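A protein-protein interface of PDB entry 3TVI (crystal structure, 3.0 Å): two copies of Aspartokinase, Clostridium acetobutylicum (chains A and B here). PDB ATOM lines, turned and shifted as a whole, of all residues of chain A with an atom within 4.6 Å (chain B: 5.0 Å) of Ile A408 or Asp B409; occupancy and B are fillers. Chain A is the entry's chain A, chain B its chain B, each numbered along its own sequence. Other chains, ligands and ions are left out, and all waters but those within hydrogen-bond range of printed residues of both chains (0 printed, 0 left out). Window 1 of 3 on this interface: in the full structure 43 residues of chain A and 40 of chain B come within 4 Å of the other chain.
Phe B395 touches its own counterpart, Phe A395. Ile A408 touches its own counterpart, Ile B408. Ile A408 touches Asp B409, and with the chains exchanged Asp A409 touches Ile B408. Ile A408 touches Gln B410, and with the chains exchanged Gln A410 touches Ile B408. Positions printed for both chains: 395, 407, 408, 409, 410, 417 and 418. Of the 13 pairs that touch across the chains among the printed residues, 8 have their exchanged pair printed and touching as well.
Among the printed residues, merely in contact across the chains: Pro A333 with Gly B411 (3.9 Å), Pro A333 with Ser B412 (3.8 Å), Ser A334 with His B331 (3.3 Å), Ser A334 with Asp B409 (3.9 Å), Ser A334 with Ser B412 (3.2 Å), Phe A395 with Phe B395 (3.8 Å), Met A407 with Gln B410 (3.3 Å), Ile A408 with Ile B408 (3.5 Å), Ile A408 with Asp B409 (3.7 Å) and Asp A409 with Ile B408 (3.7 Å).
The side-chain amide oxygen (OE1) of Gln A410 is in hydrogen-bond range of the backbone NH (N) of Met B407 (3.3 Å). The backbone NH (N) of Ile B408 sits at hydrogen-bond distance from the backbone carbonyl oxygen (O) of Gln A410 (2.7 Å). N of Ile A408 lies within hydrogen-bond range of O of Gln B410 (2.7 Å).
O of Ile A418 lies within hydrogen-bond range of N of Asp A409 (2.9 Å). OD2 of Asp B409 lies within hydrogen-bond range of OG of Ser B412 (2.4 Å). The backbone carbonyl oxygen (O) of Ile B418 sits at hydrogen-bond distance from the backbone NH (N) of Asp B409 (3.0 Å).
Of the 12 printed residues of chain B, 8 touch a printed residue of chain A. Hydrophobic or aromatic side chains of chain B that line the printed part of chain A: His B331, Phe B395, Met B407 and Ile B408. Among the printed residues, 13 pairs touch across the chains. Among the printed residues, no Asp or Glu carboxylate lies within 4 Å of a Lys or Arg side-chain nitrogen of the other chain.
Of chain B, only Ile B408 (3.5 Å), Asp B409 (3.7 Å) and Gln B410 (2.7 Å) come within 4 Å of Ile A408. Asp B409 touches just these residues of chain A: Ser A334 and Ile A408. Printed residues of chain A within 4 Å of Phe B395: Phe A395. Printed residues of chain B within 4 Å of Met A407: Gln B410. Of the printed residues of chain A, Gly B411 touches Pro A333. Of the printed residues of chain A, Met B407 touches Gln A410 (3.1 Å). Asn B416 touches none of the printed residues of chain A. Val A417 touches none of the printed residues of chain B. The nearest residue of chain B that does not touch Ile A408 is Ala B391 (4.03 Å).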
ATOM      1  N   PRO A 333       3.484 -20.915  -5.930  1.00  0.00           N
ATOM      2  CA  PRO A 333       2.925 -20.770  -4.593  1.00  0.00           C
ATOM      3  C   PRO A 333       1.463 -20.366  -4.661  1.00  0.00           C
ATOM      4  O   PRO A 333       1.101 -19.536  -5.485  1.00  0.00           O
ATOM      5  CB  PRO A 333       3.772 -19.656  -3.978  1.00  0.00           C
ATOM      6  CG  PRO A 333       5.038 -19.661  -4.761  1.00  0.00           C
ATOM      7  CD  PRO A 333       4.594 -19.976  -6.152  1.00  0.00           C
ATOM      8  N   SER A 334       0.633 -20.962  -3.818  1.00  0.00           N
ATOM      9  CA  SER A 334      -0.790 -20.648  -3.804  1.00  0.00           C
ATOM     10  C   SER A 334      -1.339 -20.752  -2.393  1.00  0.00           C
ATOM     11  O   SER A 334      -0.724 -21.385  -1.539  1.00  0.00           O
ATOM     12  CB  SER A 334      -1.542 -21.612  -4.714  1.00  0.00           C
ATOM     13  OG  SER A 334      -1.489 -22.935  -4.201  1.00  0.00           O
ATOM     14  N   PHE A 395      18.319 -21.899   7.788  1.00  0.00           N
ATOM     15  CA  PHE A 395      17.714 -20.572   7.930  1.00  0.00           C
ATOM     16  C   PHE A 395      18.273 -19.754   9.081  1.00  0.00           C
ATOM     17  O   PHE A 395      18.167 -18.526   9.079  1.00  0.00           O
ATOM     18  CB  PHE A 395      16.205 -20.695   8.037  1.00  0.00           C
ATOM     19  CG  PHE A 395      15.575 -21.202   6.786  1.00  0.00           C
ATOM     20  CD1 PHE A 395      15.468 -20.383   5.684  1.00  0.00           C
ATOM     21  CD2 PHE A 395      15.119 -22.503   6.695  1.00  0.00           C
ATOM     22  CE1 PHE A 395      14.893 -20.841   4.512  1.00  0.00           C
ATOM     23  CE2 PHE A 395      14.546 -22.975   5.527  1.00  0.00           C
ATOM     24  CZ  PHE A 395      14.434 -22.140   4.430  1.00  0.00           C
ATOM     25  N   ILE A 405      14.623 -13.469   2.926  1.00  0.00           N
ATOM     26  CA  ILE A 405      14.100 -14.605   2.178  1.00  0.00           C
ATOM     27  C   ILE A 405      12.770 -14.212   1.579  1.00  0.00           C
ATOM     28  O   ILE A 405      11.873 -13.822   2.306  1.00  0.00           O
ATOM     29  CB  ILE A 405      13.873 -15.818   3.091  1.00  0.00           C
ATOM     30  CG1 ILE A 405      15.184 -16.246   3.729  1.00  0.00           C
ATOM     31  CG2 ILE A 405      13.294 -16.981   2.307  1.00  0.00           C
ATOM     32  CD1 ILE A 405      15.026 -17.388   4.689  1.00  0.00           C
ATOM     33  N   MET A 407      11.031 -16.343  -0.611  1.00  0.00           N
ATOM     34  CA  MET A 407      10.255 -17.554  -0.872  1.00  0.00           C
ATOM     35  C   MET A 407      10.964 -18.705  -0.232  1.00  0.00           C
ATOM     36  O   MET A 407      12.190 -18.806  -0.311  1.00  0.00           O
ATOM     37  CB  MET A 407      10.167 -17.838  -2.381  1.00  0.00           C
ATOM     38  CG  MET A 407       9.151 -18.934  -2.748  1.00  0.00           C
ATOM     39  SD  MET A 407       9.511 -19.822  -4.487  1.00  0.00           S
ATOM     40  CE  MET A 407      11.246 -20.685  -4.141  1.00  0.00           C
ATOM     41  N   ILE A 408      10.209 -19.581   0.416  1.00  0.00           N
ATOM     42  CA  ILE A 408      10.700 -20.908   0.747  1.00  0.00           C
ATOM     43  C   ILE A 408       9.766 -21.923   0.144  1.00  0.00           C
ATOM     44  O   ILE A 408       8.559 -21.849   0.323  1.00  0.00           O
ATOM     45  CB  ILE A 408      10.734 -21.191   2.247  1.00  0.00           C
ATOM     46  CG1 ILE A 408      11.534 -20.124   2.993  1.00  0.00           C
ATOM     47  CG2 ILE A 408      11.320 -22.577   2.475  1.00  0.00           C
ATOM     48  CD1 ILE A 408      11.622 -20.377   4.480  1.00  0.00           C
ATOM     49  N   ASP A 409      10.327 -22.878  -0.568  1.00  0.00           N
ATOM     50  CA  ASP A 409       9.538 -23.951  -1.147  1.00  0.00           C
ATOM     51  C   ASP A 409      10.242 -25.270  -0.891  1.00  0.00           C
ATOM     52  O   ASP A 409      11.361 -25.473  -1.368  1.00  0.00           O
ATOM     53  CB  ASP A 409       9.353 -23.726  -2.652  1.00  0.00           C
ATOM     54  CG  ASP A 409       8.385 -24.716  -3.276  1.00  0.00           C
ATOM     55  OD1 ASP A 409       8.338 -25.877  -2.810  1.00  0.00           O
ATOM     56  OD2 ASP A 409       7.669 -24.336  -4.234  1.00  0.00           O
ATOM     57  N   GLN A 410       9.602 -26.139  -0.109  1.00  0.00           N
ATOM     58  CA  GLN A 410      10.071 -27.511   0.042  1.00  0.00           C
ATOM     59  C   GLN A 410       8.904 -28.418   0.342  1.00  0.00           C
ATOM     60  O   GLN A 410       8.049 -28.082   1.142  1.00  0.00           O
ATOM     61  CB  GLN A 410      11.188 -27.628   1.098  1.00  0.00           C
ATOM     62  CG  GLN A 410      10.817 -28.214   2.452  1.00  0.00           C
ATOM     63  CD  GLN A 410      10.482 -29.690   2.398  1.00  0.00           C
ATOM     64  OE1 GLN A 410       9.628 -30.146   3.141  1.00  0.00           O
ATOM     65  NE2 GLN A 410      11.136 -30.437   1.515  1.00  0.00           N
ATOM     66  N   VAL A 417      15.661 -28.436  -0.327  1.00  0.00           N
ATOM     67  CA  VAL A 417      14.972 -27.202   0.065  1.00  0.00           C
ATOM     68  C   VAL A 417      15.356 -26.102  -0.916  1.00  0.00           C
ATOM     69  O   VAL A 417      16.522 -25.989  -1.304  1.00  0.00           O
ATOM     70  CB  VAL A 417      15.358 -26.740   1.485  1.00  0.00           C
ATOM     71  CG1 VAL A 417      14.603 -25.477   1.859  1.00  0.00           C
ATOM     72  CG2 VAL A 417      15.079 -27.836   2.495  1.00  0.00           C
ATOM     73  N   ILE A 418      14.386 -25.284  -1.311  1.00  0.00           N
ATOM     74  CA  ILE A 418      14.649 -24.222  -2.276  1.00  0.00           C
ATOM     75  C   ILE A 418      14.281 -22.881  -1.675  1.00  0.00           C
ATOM     76  O   ILE A 418      13.131 -22.642  -1.333  1.00  0.00           O
ATOM     77  CB  ILE A 418      13.887 -24.441  -3.591  1.00  0.00           C
ATOM     78  CG1 ILE A 418      14.435 -25.680  -4.303  1.00  0.00           C
ATOM     79  CG2 ILE A 418      14.023 -23.225  -4.492  1.00  0.00           C
ATOM     80  CD1 ILE A 418      13.576 -26.150  -5.454  1.00  0.00           C
ATOM     81  N   HIS B 331      -1.700 -27.347  -2.287  1.00  0.00           N
ATOM     82  CA  HIS B 331      -0.460 -26.766  -2.784  1.00  0.00           C
ATOM     83  C   HIS B 331       0.154 -27.574  -3.889  1.00  0.00           C
ATOM     84  O   HIS B 331      -0.120 -28.764  -4.026  1.00  0.00           O
ATOM     85  CB  HIS B 331       0.540 -26.631  -1.637  1.00  0.00           C
ATOM     86  CG  HIS B 331       0.059 -25.743  -0.513  1.00  0.00           C
ATOM     87  ND1 HIS B 331      -0.469 -26.233   0.626  1.00  0.00           N
ATOM     88  CD2 HIS B 331       0.029 -24.357  -0.394  1.00  0.00           C
ATOM     89  CE1 HIS B 331      -0.814 -25.217   1.432  1.00  0.00           C
ATOM     90  NE2 HIS B 331      -0.508 -24.068   0.806  1.00  0.00           N
ATOM     91  N   ALA B 391      10.085 -17.421   9.800  1.00  0.00           N
ATOM     92  CA  ALA B 391       9.978 -18.857   9.516  1.00  0.00           C
ATOM     93  C   ALA B 391      10.993 -19.645  10.342  1.00  0.00           C
ATOM     94  O   ALA B 391      10.687 -20.734  10.823  1.00  0.00           O
ATOM     95  CB  ALA B 391      10.167 -19.146   8.032  1.00  0.00           C
ATOM     96  N   PHE B 395      10.791 -22.984  12.768  1.00  0.00           N
ATOM     97  CA  PHE B 395      11.561 -24.202  12.584  1.00  0.00           C
ATOM     98  C   PHE B 395      12.380 -24.514  13.824  1.00  0.00           C
ATOM     99  O   PHE B 395      12.592 -25.687  14.138  1.00  0.00           O
ATOM    100  CB  PHE B 395      12.458 -24.106  11.356  1.00  0.00           C
ATOM    101  CG  PHE B 395      11.731 -23.684  10.113  1.00  0.00           C
ATOM    102  CD1 PHE B 395      10.511 -24.247   9.782  1.00  0.00           C
ATOM    103  CD2 PHE B 395      12.271 -22.726   9.268  1.00  0.00           C
ATOM    104  CE1 PHE B 395       9.837 -23.859   8.637  1.00  0.00           C
ATOM    105  CE2 PHE B 395      11.599 -22.327   8.125  1.00  0.00           C
ATOM    106  CZ  PHE B 395      10.381 -22.897   7.807  1.00  0.00           C
ATOM    107  N   MET B 407       6.696 -30.270   4.610  1.00  0.00           N
ATOM    108  CA  MET B 407       6.483 -29.241   3.597  1.00  0.00           C
ATOM    109  C   MET B 407       6.739 -27.900   4.223  1.00  0.00           C
ATOM    110  O   MET B 407       6.536 -27.715   5.427  1.00  0.00           O
ATOM    111  CB  MET B 407       5.056 -29.307   3.042  1.00  0.00           C
ATOM    112  CG  MET B 407       4.824 -28.425   1.811  1.00  0.00           C
ATOM    113  SD  MET B 407       2.908 -27.977   1.658  1.00  0.00           S
ATOM    114  CE  MET B 407       2.951 -26.138   2.347  1.00  0.00           C
ATOM    115  N   ILE B 408       7.223 -26.969   3.411  1.00  0.00           N
ATOM    116  CA  ILE B 408       7.233 -25.561   3.757  1.00  0.00           C
ATOM    117  C   ILE B 408       6.681 -24.787   2.572  1.00  0.00           C
ATOM    118  O   ILE B 408       7.113 -24.968   1.426  1.00  0.00           O
ATOM    119  CB  ILE B 408       8.650 -25.035   4.058  1.00  0.00           C
ATOM    120  CG1 ILE B 408       9.310 -25.853   5.168  1.00  0.00           C
ATOM    121  CG2 ILE B 408       8.607 -23.566   4.461  1.00  0.00           C
ATOM    122  CD1 ILE B 408      10.757 -25.476   5.401  1.00  0.00           C
ATOM    123  N   ASP B 409       5.694 -23.950   2.851  1.00  0.00           N
ATOM    124  CA  ASP B 409       5.355 -22.867   1.949  1.00  0.00           C
ATOM    125  C   ASP B 409       5.452 -21.572   2.711  1.00  0.00           C
ATOM    126  O   ASP B 409       4.739 -21.353   3.695  1.00  0.00           O
ATOM    127  CB  ASP B 409       3.949 -22.996   1.370  1.00  0.00           C
ATOM    128  CG  ASP B 409       3.457 -21.693   0.725  1.00  0.00           C
ATOM    129  OD1 ASP B 409       4.253 -21.014   0.019  1.00  0.00           O
ATOM    130  OD2 ASP B 409       2.271 -21.354   0.941  1.00  0.00           O
ATOM    131  N   GLN B 410       6.352 -20.718   2.249  1.00  0.00           N
ATOM    132  CA  GLN B 410       6.307 -19.320   2.609  1.00  0.00           C
ATOM    133  C   GLN B 410       6.651 -18.594   1.329  1.00  0.00           C
ATOM    134  O   GLN B 410       7.687 -18.828   0.735  1.00  0.00           O
ATOM    135  CB  GLN B 410       7.215 -19.038   3.809  1.00  0.00           C
ATOM    136  CG  GLN B 410       8.582 -18.440   3.566  1.00  0.00           C
ATOM    137  CD  GLN B 410       8.593 -16.965   3.847  1.00  0.00           C
ATOM    138  OE1 GLN B 410       9.297 -16.493   4.745  1.00  0.00           O
ATOM    139  NE2 GLN B 410       7.783 -16.223   3.103  1.00  0.00           N
ATOM    140  N   GLY B 411       5.724 -17.768   0.871  1.00  0.00           N
ATOM    141  CA  GLY B 411       5.769 -17.250  -0.491  1.00  0.00           C
ATOM    142  C   GLY B 411       4.386 -17.124  -1.099  1.00  0.00           C
ATOM    143  O   GLY B 411       4.168 -16.291  -1.979  1.00  0.00           O
ATOM    144  N   SER B 412       3.444 -17.945  -0.641  1.00  0.00           N
ATOM    145  CA  SER B 412       2.064 -17.817  -1.102  1.00  0.00           C
ATOM    146  C   SER B 412       1.428 -16.530  -0.590  1.00  0.00           C
ATOM    147  O   SER B 412       0.600 -15.949  -1.277  1.00  0.00           O
ATOM    148  CB  SER B 412       1.214 -19.019  -0.688  1.00  0.00           C
ATOM    149  OG  SER B 412       1.214 -19.198   0.716  1.00  0.00           O
ATOM    150  N   ASN B 416       1.791 -15.142   6.357  1.00  0.00           N
ATOM    151  CA  ASN B 416       1.449 -16.549   6.542  1.00  0.00           C
ATOM    152  C   ASN B 416       2.537 -17.556   6.162  1.00  0.00           C
ATOM    153  O   ASN B 416       2.926 -17.638   5.004  1.00  0.00           O
ATOM    154  CB  ASN B 416       0.178 -16.802   5.726  1.00  0.00           C
ATOM    155  CG  ASN B 416      -0.061 -18.260   5.428  1.00  0.00           C
ATOM    156  OD1 ASN B 416      -0.293 -19.057   6.330  1.00  0.00           O
ATOM    157  ND2 ASN B 416      -0.043 -18.610   4.150  1.00  0.00           N
ATOM    158  N   VAL B 417       3.016 -18.323   7.140  1.00  0.00           N
ATOM    159  CA  VAL B 417       3.864 -19.493   6.855  1.00  0.00           C
ATOM    160  C   VAL B 417       3.114 -20.788   7.145  1.00  0.00           C
ATOM    161  O   VAL B 417       2.556 -20.967   8.237  1.00  0.00           O
ATOM    162  CB  VAL B 417       5.172 -19.527   7.669  1.00  0.00           C
ATOM    163  CG1 VAL B 417       5.950 -20.793   7.344  1.00  0.00           C
ATOM    164  CG2 VAL B 417       6.014 -18.304   7.370  1.00  0.00           C
ATOM    165  N   ILE B 418       3.126 -21.690   6.165  1.00  0.00           N
ATOM    166  CA  ILE B 418       2.492 -22.985   6.295  1.00  0.00           C
ATOM    167  C   ILE B 418       3.563 -24.061   6.348  1.00  0.00           C
ATOM    168  O   ILE B 418       4.493 -24.084   5.543  1.00  0.00           O
ATOM    169  CB  ILE B 418       1.552 -23.277   5.124  1.00  0.00           C
ATOM    170  CG1 ILE B 418       0.495 -22.181   5.003  1.00  0.00           C
ATOM    171  CG2 ILE B 418       0.884 -24.628   5.319  1.00  0.00           C
ATOM    172  CD1 ILE B 418       0.347 -21.678   3.581  1.00  0.00           C
